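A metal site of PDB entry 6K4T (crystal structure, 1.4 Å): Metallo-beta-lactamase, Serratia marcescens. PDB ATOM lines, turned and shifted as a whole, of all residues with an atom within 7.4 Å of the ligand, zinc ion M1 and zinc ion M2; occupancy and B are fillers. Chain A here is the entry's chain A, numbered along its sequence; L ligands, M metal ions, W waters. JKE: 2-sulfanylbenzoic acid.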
ATOM      1  N   TRP A   5     -29.749 -18.329  -6.751  1.00  0.00           N
ATOM      2  CA  TRP A   5     -29.349 -18.476  -8.148  1.00  0.00           C
ATOM      3  C   TRP A   5     -30.096 -19.626  -8.830  1.00  0.00           C
ATOM      4  O   TRP A   5     -30.176 -19.698 -10.037  1.00  0.00           O
ATOM      5  CB  TRP A   5     -27.861 -18.769  -8.276  1.00  0.00           C
ATOM      6  CG  TRP A   5     -26.952 -17.648  -7.905  1.00  0.00           C
ATOM      7  CD1 TRP A   5     -27.269 -16.336  -7.736  1.00  0.00           C
ATOM      8  CD2 TRP A   5     -25.545 -17.773  -7.672  1.00  0.00           C
ATOM      9  NE1 TRP A   5     -26.144 -15.618  -7.446  1.00  0.00           N
ATOM     10  CE2 TRP A   5     -25.073 -16.474  -7.383  1.00  0.00           C
ATOM     11  CE3 TRP A   5     -24.657 -18.843  -7.684  1.00  0.00           C
ATOM     12  CZ2 TRP A   5     -23.743 -16.232  -7.091  1.00  0.00           C
ATOM     13  CZ3 TRP A   5     -23.326 -18.602  -7.392  1.00  0.00           C
ATOM     14  CH2 TRP A   5     -22.885 -17.309  -7.110  1.00  0.00           C
ATOM     15  N   GLY A  25     -32.759 -15.617  -9.211  1.00  0.00           N
ATOM     16  CA  GLY A  25     -31.523 -14.861  -8.996  1.00  0.00           C
ATOM     17  C   GLY A  25     -30.630 -14.702 -10.227  1.00  0.00           C
ATOM     18  O   GLY A  25     -29.682 -13.936 -10.170  1.00  0.00           O
ATOM     19  N   ILE A  26     -30.870 -15.479 -11.290  1.00  0.00           N
ATOM     20  CA  ILE A  26     -30.039 -15.420 -12.484  1.00  0.00           C
ATOM     21  C   ILE A  26     -30.918 -15.341 -13.720  1.00  0.00           C
ATOM     22  O   ILE A  26     -31.825 -16.158 -13.920  1.00  0.00           O
ATOM     23  CB  ILE A  26     -29.061 -16.614 -12.613  1.00  0.00           C
ATOM     24  CG1 ILE A  26     -28.152 -16.700 -11.385  1.00  0.00           C
ATOM     25  CG2 ILE A  26     -28.269 -16.529 -13.898  1.00  0.00           C
ATOM     26  CD1 ILE A  26     -27.080 -15.643 -11.377  1.00  0.00           C
ATOM     27  N   HIS A  72     -21.122 -15.197 -19.988  1.00  0.00           N
ATOM     28  CA  HIS A  72     -19.809 -15.583 -19.583  1.00  0.00           C
ATOM     29  C   HIS A  72     -19.820 -16.879 -18.778  1.00  0.00           C
ATOM     30  O   HIS A  72     -20.849 -17.322 -18.277  1.00  0.00           O
ATOM     31  CB  HIS A  72     -19.113 -14.457 -18.811  1.00  0.00           C
ATOM     32  CG  HIS A  72     -19.603 -14.225 -17.411  1.00  0.00           C
ATOM     33  ND1 HIS A  72     -20.606 -13.322 -17.110  1.00  0.00           N
ATOM     34  CD2 HIS A  72     -19.199 -14.750 -16.228  1.00  0.00           C
ATOM     35  CE1 HIS A  72     -20.807 -13.322 -15.796  1.00  0.00           C
ATOM     36  NE2 HIS A  72     -19.941 -14.185 -15.225  1.00  0.00           N
ATOM     37  N   SER A  73     -18.607 -17.428 -18.658  1.00  0.00           N
ATOM     38  CA  SER A  73     -18.386 -18.801 -18.243  1.00  0.00           C
ATOM     39  C   SER A  73     -18.069 -18.894 -16.737  1.00  0.00           C
ATOM     40  O   SER A  73     -16.997 -19.353 -16.373  1.00  0.00           O
ATOM     41  CB  SER A  73     -17.285 -19.384 -19.081  1.00  0.00           C
ATOM     42  OG  SER A  73     -16.174 -18.486 -19.143  1.00  0.00           O
ATOM     43  N   HIS A  74     -19.012 -18.447 -15.897  1.00  0.00           N
ATOM     44  CA  HIS A  74     -18.998 -18.788 -14.461  1.00  0.00           C
ATOM     45  C   HIS A  74     -20.210 -19.661 -14.122  1.00  0.00           C
ATOM     46  O   HIS A  74     -21.224 -19.654 -14.832  1.00  0.00           O
ATOM     47  CB  HIS A  74     -18.981 -17.526 -13.583  1.00  0.00           C
ATOM     48  CG  HIS A  74     -17.722 -16.754 -13.721  1.00  0.00           C
ATOM     49  ND1 HIS A  74     -17.629 -15.399 -13.496  1.00  0.00           N
ATOM     50  CD2 HIS A  74     -16.493 -17.161 -14.096  1.00  0.00           C
ATOM     51  CE1 HIS A  74     -16.383 -15.028 -13.702  1.00  0.00           C
ATOM     52  NE2 HIS A  74     -15.671 -16.072 -14.089  1.00  0.00           N
ATOM     53  N   GLU A  75     -20.108 -20.399 -13.015  1.00  0.00           N
ATOM     54  CA  GLU A  75     -21.092 -21.417 -12.666  1.00  0.00           C
ATOM     55  C   GLU A  75     -22.516 -20.832 -12.589  1.00  0.00           C
ATOM     56  O   GLU A  75     -23.463 -21.583 -12.822  1.00  0.00           O
ATOM     57  CB  GLU A  75     -20.701 -22.110 -11.356  1.00  0.00           C
ATOM     58  CG  GLU A  75     -20.771 -21.216 -10.127  1.00  0.00           C
ATOM     59  CD  GLU A  75     -20.470 -21.840  -8.772  1.00  0.00           C
ATOM     60  OE1 GLU A  75     -20.894 -22.971  -8.551  1.00  0.00           O
ATOM     61  OE2 GLU A  75     -19.859 -21.155  -7.922  1.00  0.00           O
ATOM     62  N   ASP A  76     -22.676 -19.566 -12.200  1.00  0.00           N
ATOM     63  CA  ASP A  76     -24.002 -19.041 -11.934  1.00  0.00           C
ATOM     64  C   ASP A  76     -24.779 -18.776 -13.231  1.00  0.00           C
ATOM     65  O   ASP A  76     -25.990 -18.849 -13.217  1.00  0.00           O
ATOM     66  CB  ASP A  76     -23.937 -17.838 -10.987  1.00  0.00           C
ATOM     67  CG  ASP A  76     -23.041 -16.695 -11.437  1.00  0.00           C
ATOM     68  OD1 ASP A  76     -22.038 -16.957 -12.134  1.00  0.00           O
ATOM     69  OD2 ASP A  76     -23.391 -15.524 -11.112  1.00  0.00           O
ATOM     70  N   HIS A  77     -24.086 -18.465 -14.330  1.00  0.00           N
ATOM     71  CA  HIS A  77     -24.711 -18.172 -15.639  1.00  0.00           C
ATOM     72  C   HIS A  77     -24.667 -19.406 -16.557  1.00  0.00           C
ATOM     73  O   HIS A  77     -25.552 -19.592 -17.402  1.00  0.00           O
ATOM     74  CB  HIS A  77     -24.063 -16.967 -16.308  1.00  0.00           C
ATOM     75  CG  HIS A  77     -23.958 -15.807 -15.363  1.00  0.00           C
ATOM     76  ND1 HIS A  77     -25.051 -14.973 -15.094  1.00  0.00           N
ATOM     77  CD2 HIS A  77     -22.940 -15.393 -14.577  1.00  0.00           C
ATOM     78  CE1 HIS A  77     -24.669 -14.091 -14.180  1.00  0.00           C
ATOM     79  NE2 HIS A  77     -23.395 -14.340 -13.805  1.00  0.00           N
ATOM     80  N   ASP A 111      -8.560 -15.301 -15.428  1.00  0.00           N
ATOM     81  CA  ASP A 111      -9.770 -14.801 -14.786  1.00  0.00           C
ATOM     82  C   ASP A 111      -9.405 -14.164 -13.444  1.00  0.00           C
ATOM     83  O   ASP A 111      -8.759 -14.802 -12.632  1.00  0.00           O
ATOM     84  CB  ASP A 111     -10.784 -15.929 -14.648  1.00  0.00           C
ATOM     85  CG  ASP A 111     -12.173 -15.495 -14.216  1.00  0.00           C
ATOM     86  OD1 ASP A 111     -12.283 -14.738 -13.227  1.00  0.00           O
ATOM     87  OD2 ASP A 111     -13.123 -15.974 -14.834  1.00  0.00           O
ATOM     88  N   GLN A 113     -10.955 -13.913 -10.800  1.00  0.00           N
ATOM     89  CA  GLN A 113     -11.453 -14.737  -9.695  1.00  0.00           C
ATOM     90  C   GLN A 113     -10.739 -16.079  -9.607  1.00  0.00           C
ATOM     91  O   GLN A 113     -11.025 -16.853  -8.696  1.00  0.00           O
ATOM     92  CB  GLN A 113     -12.965 -14.935  -9.809  1.00  0.00           C
ATOM     93  CG  GLN A 113     -13.743 -13.643  -9.553  1.00  0.00           C
ATOM     94  CD  GLN A 113     -15.224 -13.876  -9.690  1.00  0.00           C
ATOM     95  OE1 GLN A 113     -15.823 -13.666 -10.748  1.00  0.00           O
ATOM     96  NE2 GLN A 113     -15.819 -14.412  -8.643  1.00  0.00           N
ATOM     97  N   LEU A 117     -13.023 -19.675  -7.808  1.00  0.00           N
ATOM     98  CA  LEU A 117     -14.191 -20.081  -8.587  1.00  0.00           C
ATOM     99  C   LEU A 117     -14.499 -21.560  -8.359  1.00  0.00           C
ATOM    100  O   LEU A 117     -13.600 -22.359  -8.132  1.00  0.00           O
ATOM    101  CB  LEU A 117     -13.946 -19.811 -10.080  1.00  0.00           C
ATOM    102  CG  LEU A 117     -13.906 -18.322 -10.451  1.00  0.00           C
ATOM    103  CD1 LEU A 117     -13.222 -18.106 -11.802  1.00  0.00           C
ATOM    104  CD2 LEU A 117     -15.300 -17.727 -10.451  1.00  0.00           C
ATOM    105  N   HIS A 150     -14.697  -8.911 -17.085  1.00  0.00           N
ATOM    106  CA  HIS A 150     -15.116  -9.880 -16.064  1.00  0.00           C
ATOM    107  C   HIS A 150     -14.608 -11.270 -16.433  1.00  0.00           C
ATOM    108  O   HIS A 150     -14.164 -12.015 -15.564  1.00  0.00           O
ATOM    109  CB  HIS A 150     -16.637  -9.775 -15.846  1.00  0.00           C
ATOM    110  CG  HIS A 150     -17.176 -10.666 -14.787  1.00  0.00           C
ATOM    111  ND1 HIS A 150     -17.154 -10.324 -13.447  1.00  0.00           N
ATOM    112  CD2 HIS A 150     -17.789 -11.867 -14.853  1.00  0.00           C
ATOM    113  CE1 HIS A 150     -17.750 -11.277 -12.738  1.00  0.00           C
ATOM    114  NE2 HIS A 150     -18.153 -12.232 -13.585  1.00  0.00           N
ATOM    115  N   THR A 151     -14.661 -11.572 -17.742  1.00  0.00           N
ATOM    116  CA  THR A 151     -13.988 -12.741 -18.355  1.00  0.00           C
ATOM    117  C   THR A 151     -13.471 -12.288 -19.718  1.00  0.00           C
ATOM    118  O   THR A 151     -13.986 -11.302 -20.265  1.00  0.00           O
ATOM    119  CB  THR A 151     -14.920 -13.948 -18.524  1.00  0.00           C
ATOM    120  OG1 THR A 151     -15.918 -13.617 -19.502  1.00  0.00           O
ATOM    121  CG2 THR A 151     -15.546 -14.424 -17.235  1.00  0.00           C
ATOM    122  N   ASP A 174     -24.118  -8.686 -20.338  1.00  0.00           N
ATOM    123  CA  ASP A 174     -23.132  -9.425 -19.570  1.00  0.00           C
ATOM    124  C   ASP A 174     -22.693  -8.585 -18.360  1.00  0.00           C
ATOM    125  O   ASP A 174     -22.880  -7.354 -18.306  1.00  0.00           O
ATOM    126  CB  ASP A 174     -21.939  -9.796 -20.425  1.00  0.00           C
ATOM    127  CG  ASP A 174     -21.005 -10.798 -19.768  1.00  0.00           C
ATOM    128  OD1 ASP A 174     -21.471 -11.520 -18.863  1.00  0.00           O
ATOM    129  OD2 ASP A 174     -19.862 -10.922 -20.266  1.00  0.00           O
ATOM    130  N   SER A 175     -22.170  -9.294 -17.361  1.00  0.00           N
ATOM    131  CA  SER A 175     -21.573  -8.660 -16.194  1.00  0.00           C
ATOM    132  C   SER A 175     -20.330  -7.855 -16.579  1.00  0.00           C
ATOM    133  O   SER A 175     -19.489  -8.319 -17.335  1.00  0.00           O
ATOM    134  CB  SER A 175     -21.253  -9.714 -15.177  1.00  0.00           C
ATOM    135  OG  SER A 175     -22.433 -10.432 -14.845  1.00  0.00           O
ATOM    136  N   LEU A 176     -20.202  -6.651 -16.014  1.00  0.00           N
ATOM    137  CA  LEU A 176     -19.090  -5.760 -16.247  1.00  0.00           C
ATOM    138  C   LEU A 176     -18.318  -5.508 -14.947  1.00  0.00           C
ATOM    139  O   LEU A 176     -17.738  -4.426 -14.759  1.00  0.00           O
ATOM    140  CB  LEU A 176     -19.651  -4.441 -16.787  1.00  0.00           C
ATOM    141  CG  LEU A 176     -20.491  -4.517 -18.058  1.00  0.00           C
ATOM    142  CD1 LEU A 176     -20.942  -3.139 -18.517  1.00  0.00           C
ATOM    143  CD2 LEU A 176     -19.720  -5.225 -19.159  1.00  0.00           C
ATOM    144  N   THR A 177     -18.367  -6.456 -14.013  1.00  0.00           N
ATOM    145  CA  THR A 177     -17.926  -6.239 -12.655  1.00  0.00           C
ATOM    146  C   THR A 177     -16.473  -6.682 -12.428  1.00  0.00           C
ATOM    147  O   THR A 177     -16.042  -7.776 -12.742  1.00  0.00           O
ATOM    148  CB  THR A 177     -18.833  -7.022 -11.707  1.00  0.00           C
ATOM    149  OG1 THR A 177     -18.804  -8.399 -12.116  1.00  0.00           O
ATOM    150  CG2 THR A 177     -20.257  -6.505 -11.704  1.00  0.00           C
ATOM    151  N   ALA A 178     -15.718  -5.777 -11.793  1.00  0.00           N
ATOM    152  CA  ALA A 178     -14.385  -6.034 -11.262  1.00  0.00           C
ATOM    153  C   ALA A 178     -14.514  -6.717  -9.906  1.00  0.00           C
ATOM    154  O   ALA A 178     -14.906  -6.079  -8.890  1.00  0.00           O
ATOM    155  CB  ALA A 178     -13.612  -4.737 -11.175  1.00  0.00           C
ATOM    156  N   VAL A 179     -14.228  -8.016  -9.898  1.00  0.00           N
ATOM    157  CA  VAL A 179     -14.258  -8.849  -8.690  1.00  0.00           C
ATOM    158  C   VAL A 179     -13.097  -9.839  -8.831  1.00  0.00           C
ATOM    159  O   VAL A 179     -12.783 -10.246  -9.908  1.00  0.00           O
ATOM    160  CB  VAL A 179     -15.627  -9.563  -8.537  1.00  0.00           C
ATOM    161  CG1 VAL A 179     -16.044 -10.295  -9.791  1.00  0.00           C
ATOM    162  CG2 VAL A 179     -15.688 -10.508  -7.348  1.00  0.00           C
ATOM    163  N   SER A 180     -12.511 -10.256  -7.719  1.00  0.00           N
ATOM    164  CA  SER A 180     -11.309 -11.092  -7.823  1.00  0.00           C
ATOM    165  C   SER A 180     -11.099 -11.950  -6.579  1.00  0.00           C
ATOM    166  O   SER A 180     -11.686 -11.695  -5.511  1.00  0.00           O
ATOM    167  CB  SER A 180     -10.068 -10.259  -8.072  1.00  0.00           C
ATOM    168  OG  SER A 180      -9.651  -9.610  -6.864  1.00  0.00           O
ATOM    169  N   ALA A 214     -27.494  -9.945 -16.610  1.00  0.00           N
ATOM    170  CA  ALA A 214     -27.252 -11.350 -16.275  1.00  0.00           C
ATOM    171  C   ALA A 214     -27.628 -11.639 -14.804  1.00  0.00           C
ATOM    172  O   ALA A 214     -28.261 -12.658 -14.509  1.00  0.00           O
ATOM    173  CB  ALA A 214     -25.803 -11.693 -16.546  1.00  0.00           C
ATOM    174  N   HIS A 215     -27.235 -10.735 -13.897  1.00  0.00           N
ATOM    175  CA  HIS A 215     -27.816 -10.647 -12.567  1.00  0.00           C
ATOM    176  C   HIS A 215     -29.005  -9.698 -12.634  1.00  0.00           C
ATOM    177  O   HIS A 215     -28.790  -8.496 -12.798  1.00  0.00           O
ATOM    178  CB  HIS A 215     -26.769 -10.174 -11.538  1.00  0.00           C
ATOM    179  CG  HIS A 215     -25.753 -11.239 -11.244  1.00  0.00           C
ATOM    180  ND1 HIS A 215     -25.992 -12.227 -10.314  1.00  0.00           N
ATOM    181  CD2 HIS A 215     -24.552 -11.524 -11.799  1.00  0.00           C
ATOM    182  CE1 HIS A 215     -24.981 -13.066 -10.293  1.00  0.00           C
ATOM    183  NE2 HIS A 215     -24.059 -12.653 -11.187  1.00  0.00           N
ATOM    184  N   VAL A 218     -29.427  -6.073 -11.286  1.00  0.00           N
ATOM    185  CA  VAL A 218     -28.541  -5.041 -11.769  1.00  0.00           C
ATOM    186  C   VAL A 218     -29.333  -3.939 -12.477  1.00  0.00           C
ATOM    187  O   VAL A 218     -28.981  -2.765 -12.371  1.00  0.00           O
ATOM    188  CB  VAL A 218     -27.410  -5.630 -12.642  1.00  0.00           C
ATOM    189  CG1 VAL A 218     -26.751  -4.584 -13.530  1.00  0.00           C
ATOM    190  CG2 VAL A 218     -26.365  -6.275 -11.756  1.00  0.00           C
ATOM    191  N   ARG A 252     -17.454   0.650  -9.955  1.00  0.00           N
ATOM    192  CA  ARG A 252     -16.882  -0.479  -9.236  1.00  0.00           C
ATOM    193  C   ARG A 252     -15.381  -0.602  -9.518  1.00  0.00           C
ATOM    194  O   ARG A 252     -14.571  -0.836  -8.615  1.00  0.00           O
ATOM    195  CB  ARG A 252     -17.613  -1.756  -9.626  1.00  0.00           C
ATOM    196  CG  ARG A 252     -17.193  -2.999  -8.843  1.00  0.00           C
ATOM    197  CD  ARG A 252     -18.173  -4.125  -9.072  1.00  0.00           C
ATOM    198  NE  ARG A 252     -17.743  -5.323  -8.358  1.00  0.00           N
ATOM    199  CZ  ARG A 252     -18.557  -6.257  -7.855  1.00  0.00           C
ATOM    200  NH1 ARG A 252     -19.854  -6.210  -8.126  1.00  0.00           N
ATOM    201  NH2 ARG A 252     -18.074  -7.277  -7.182  1.00  0.00           N
HETATM  202  SD  JKE L   1     -20.373 -14.203 -11.443  1.00  0.00           S
HETATM  203  CG  JKE L   1     -21.115 -11.026 -11.851  1.00  0.00           C
HETATM  204  CZ  JKE L   1     -20.411 -11.506 -10.642  1.00  0.00           C
HETATM  205  CD1 JKE L   1     -19.332 -13.197  -9.194  1.00  0.00           C
HETATM  206  OD1 JKE L   1     -21.191  -9.808 -12.002  1.00  0.00           O
HETATM  207  CD2 JKE L   1     -19.442 -10.898  -8.504  1.00  0.00           C
HETATM  208  OD2 JKE L   1     -21.647 -11.838 -12.721  1.00  0.00           O
HETATM  209  CE1 JKE L   1     -20.008 -12.888 -10.382  1.00  0.00           C
HETATM  210  CE2 JKE L   1     -20.119 -10.555  -9.669  1.00  0.00           C
HETATM  211  CG1 JKE L   1     -19.039 -12.201  -8.261  1.00  0.00           C
HETATM  212 ZN    ZN M   1     -22.615 -13.862 -12.035  1.00  0.00          ZN
HETATM  213 ZN    ZN M   2     -19.185 -13.988 -13.333  1.00  0.00          ZN
HETATM  214  O   HOH W   1     -23.196 -10.956  -8.229  1.00  0.00           O
HETATM  215  O   HOH W   2     -23.185  -7.872 -12.563  1.00  0.00           O
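The nearest printed residue that does not touch zinc ion M1 is His 72 (4.2 Å).
Zinc ion M2 is bound by a ring nitrogen (NE2) of His 72, a ring nitrogen (NE2) of His 150, a ring nitrogen (ND1) of His 74 and a sulfur (SD) of the ligand.
OG of Ser 175 lies within hydrogen-bond range of OD1 of the ligand, at 3.2 Å.
The side-chain hydroxyl of Thr 177 is in hydrogen-bond range of an oxygen (OD1) of the ligand, at 2.8 Å.
OD1 of Asp 174 is in hydrogen-bond range of ND1 of His 72 (2.7 Å).
A ring nitrogen (ND1) of His 150 is in hydrogen-bond range of the side-chain hydroxyl (OG1) of Thr 177.
The backbone NH of Gln 113 lies within hydrogen-bond range of the side-chain carboxylate of Asp 111 (2.9 Å).
NE2 of His 74 lies within hydrogen-bond range of OD2 of Asp 111 (2.7 Å).
Residues that only touch the ligand: Val 179 and Gln 113.
Hydrophobic or aromatic side chains within 4 Å of the ligand: His 72, His 150, Val 179 and His 215.
Ten residues have an atom within 4 Å of the ligand: His 72, His 74, Asp 76, His 77, Gln 113, His 150, Ser 175, Thr 177, Val 179 and His 215.
The nearest printed residue that does not touch the ligand is Arg 252 (4.1 Å).
Zinc ion M1 is bound by a ring nitrogen (NE2) of His 77 (2.0 Å), the side-chain carboxylate of Asp 76 (2.1 Å), a ring nitrogen (NE2) of His 215 (2.1 Å), a sulfur (SD) of the ligand (2.3 Å) and an oxygen (OD2) of the ligand (2.3 Å).
Zinc ion M1 has five donor atoms within binding distance.
Three residues have an atom within 4 Å of zinc ion M2: His 72, His 74 and His 150.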
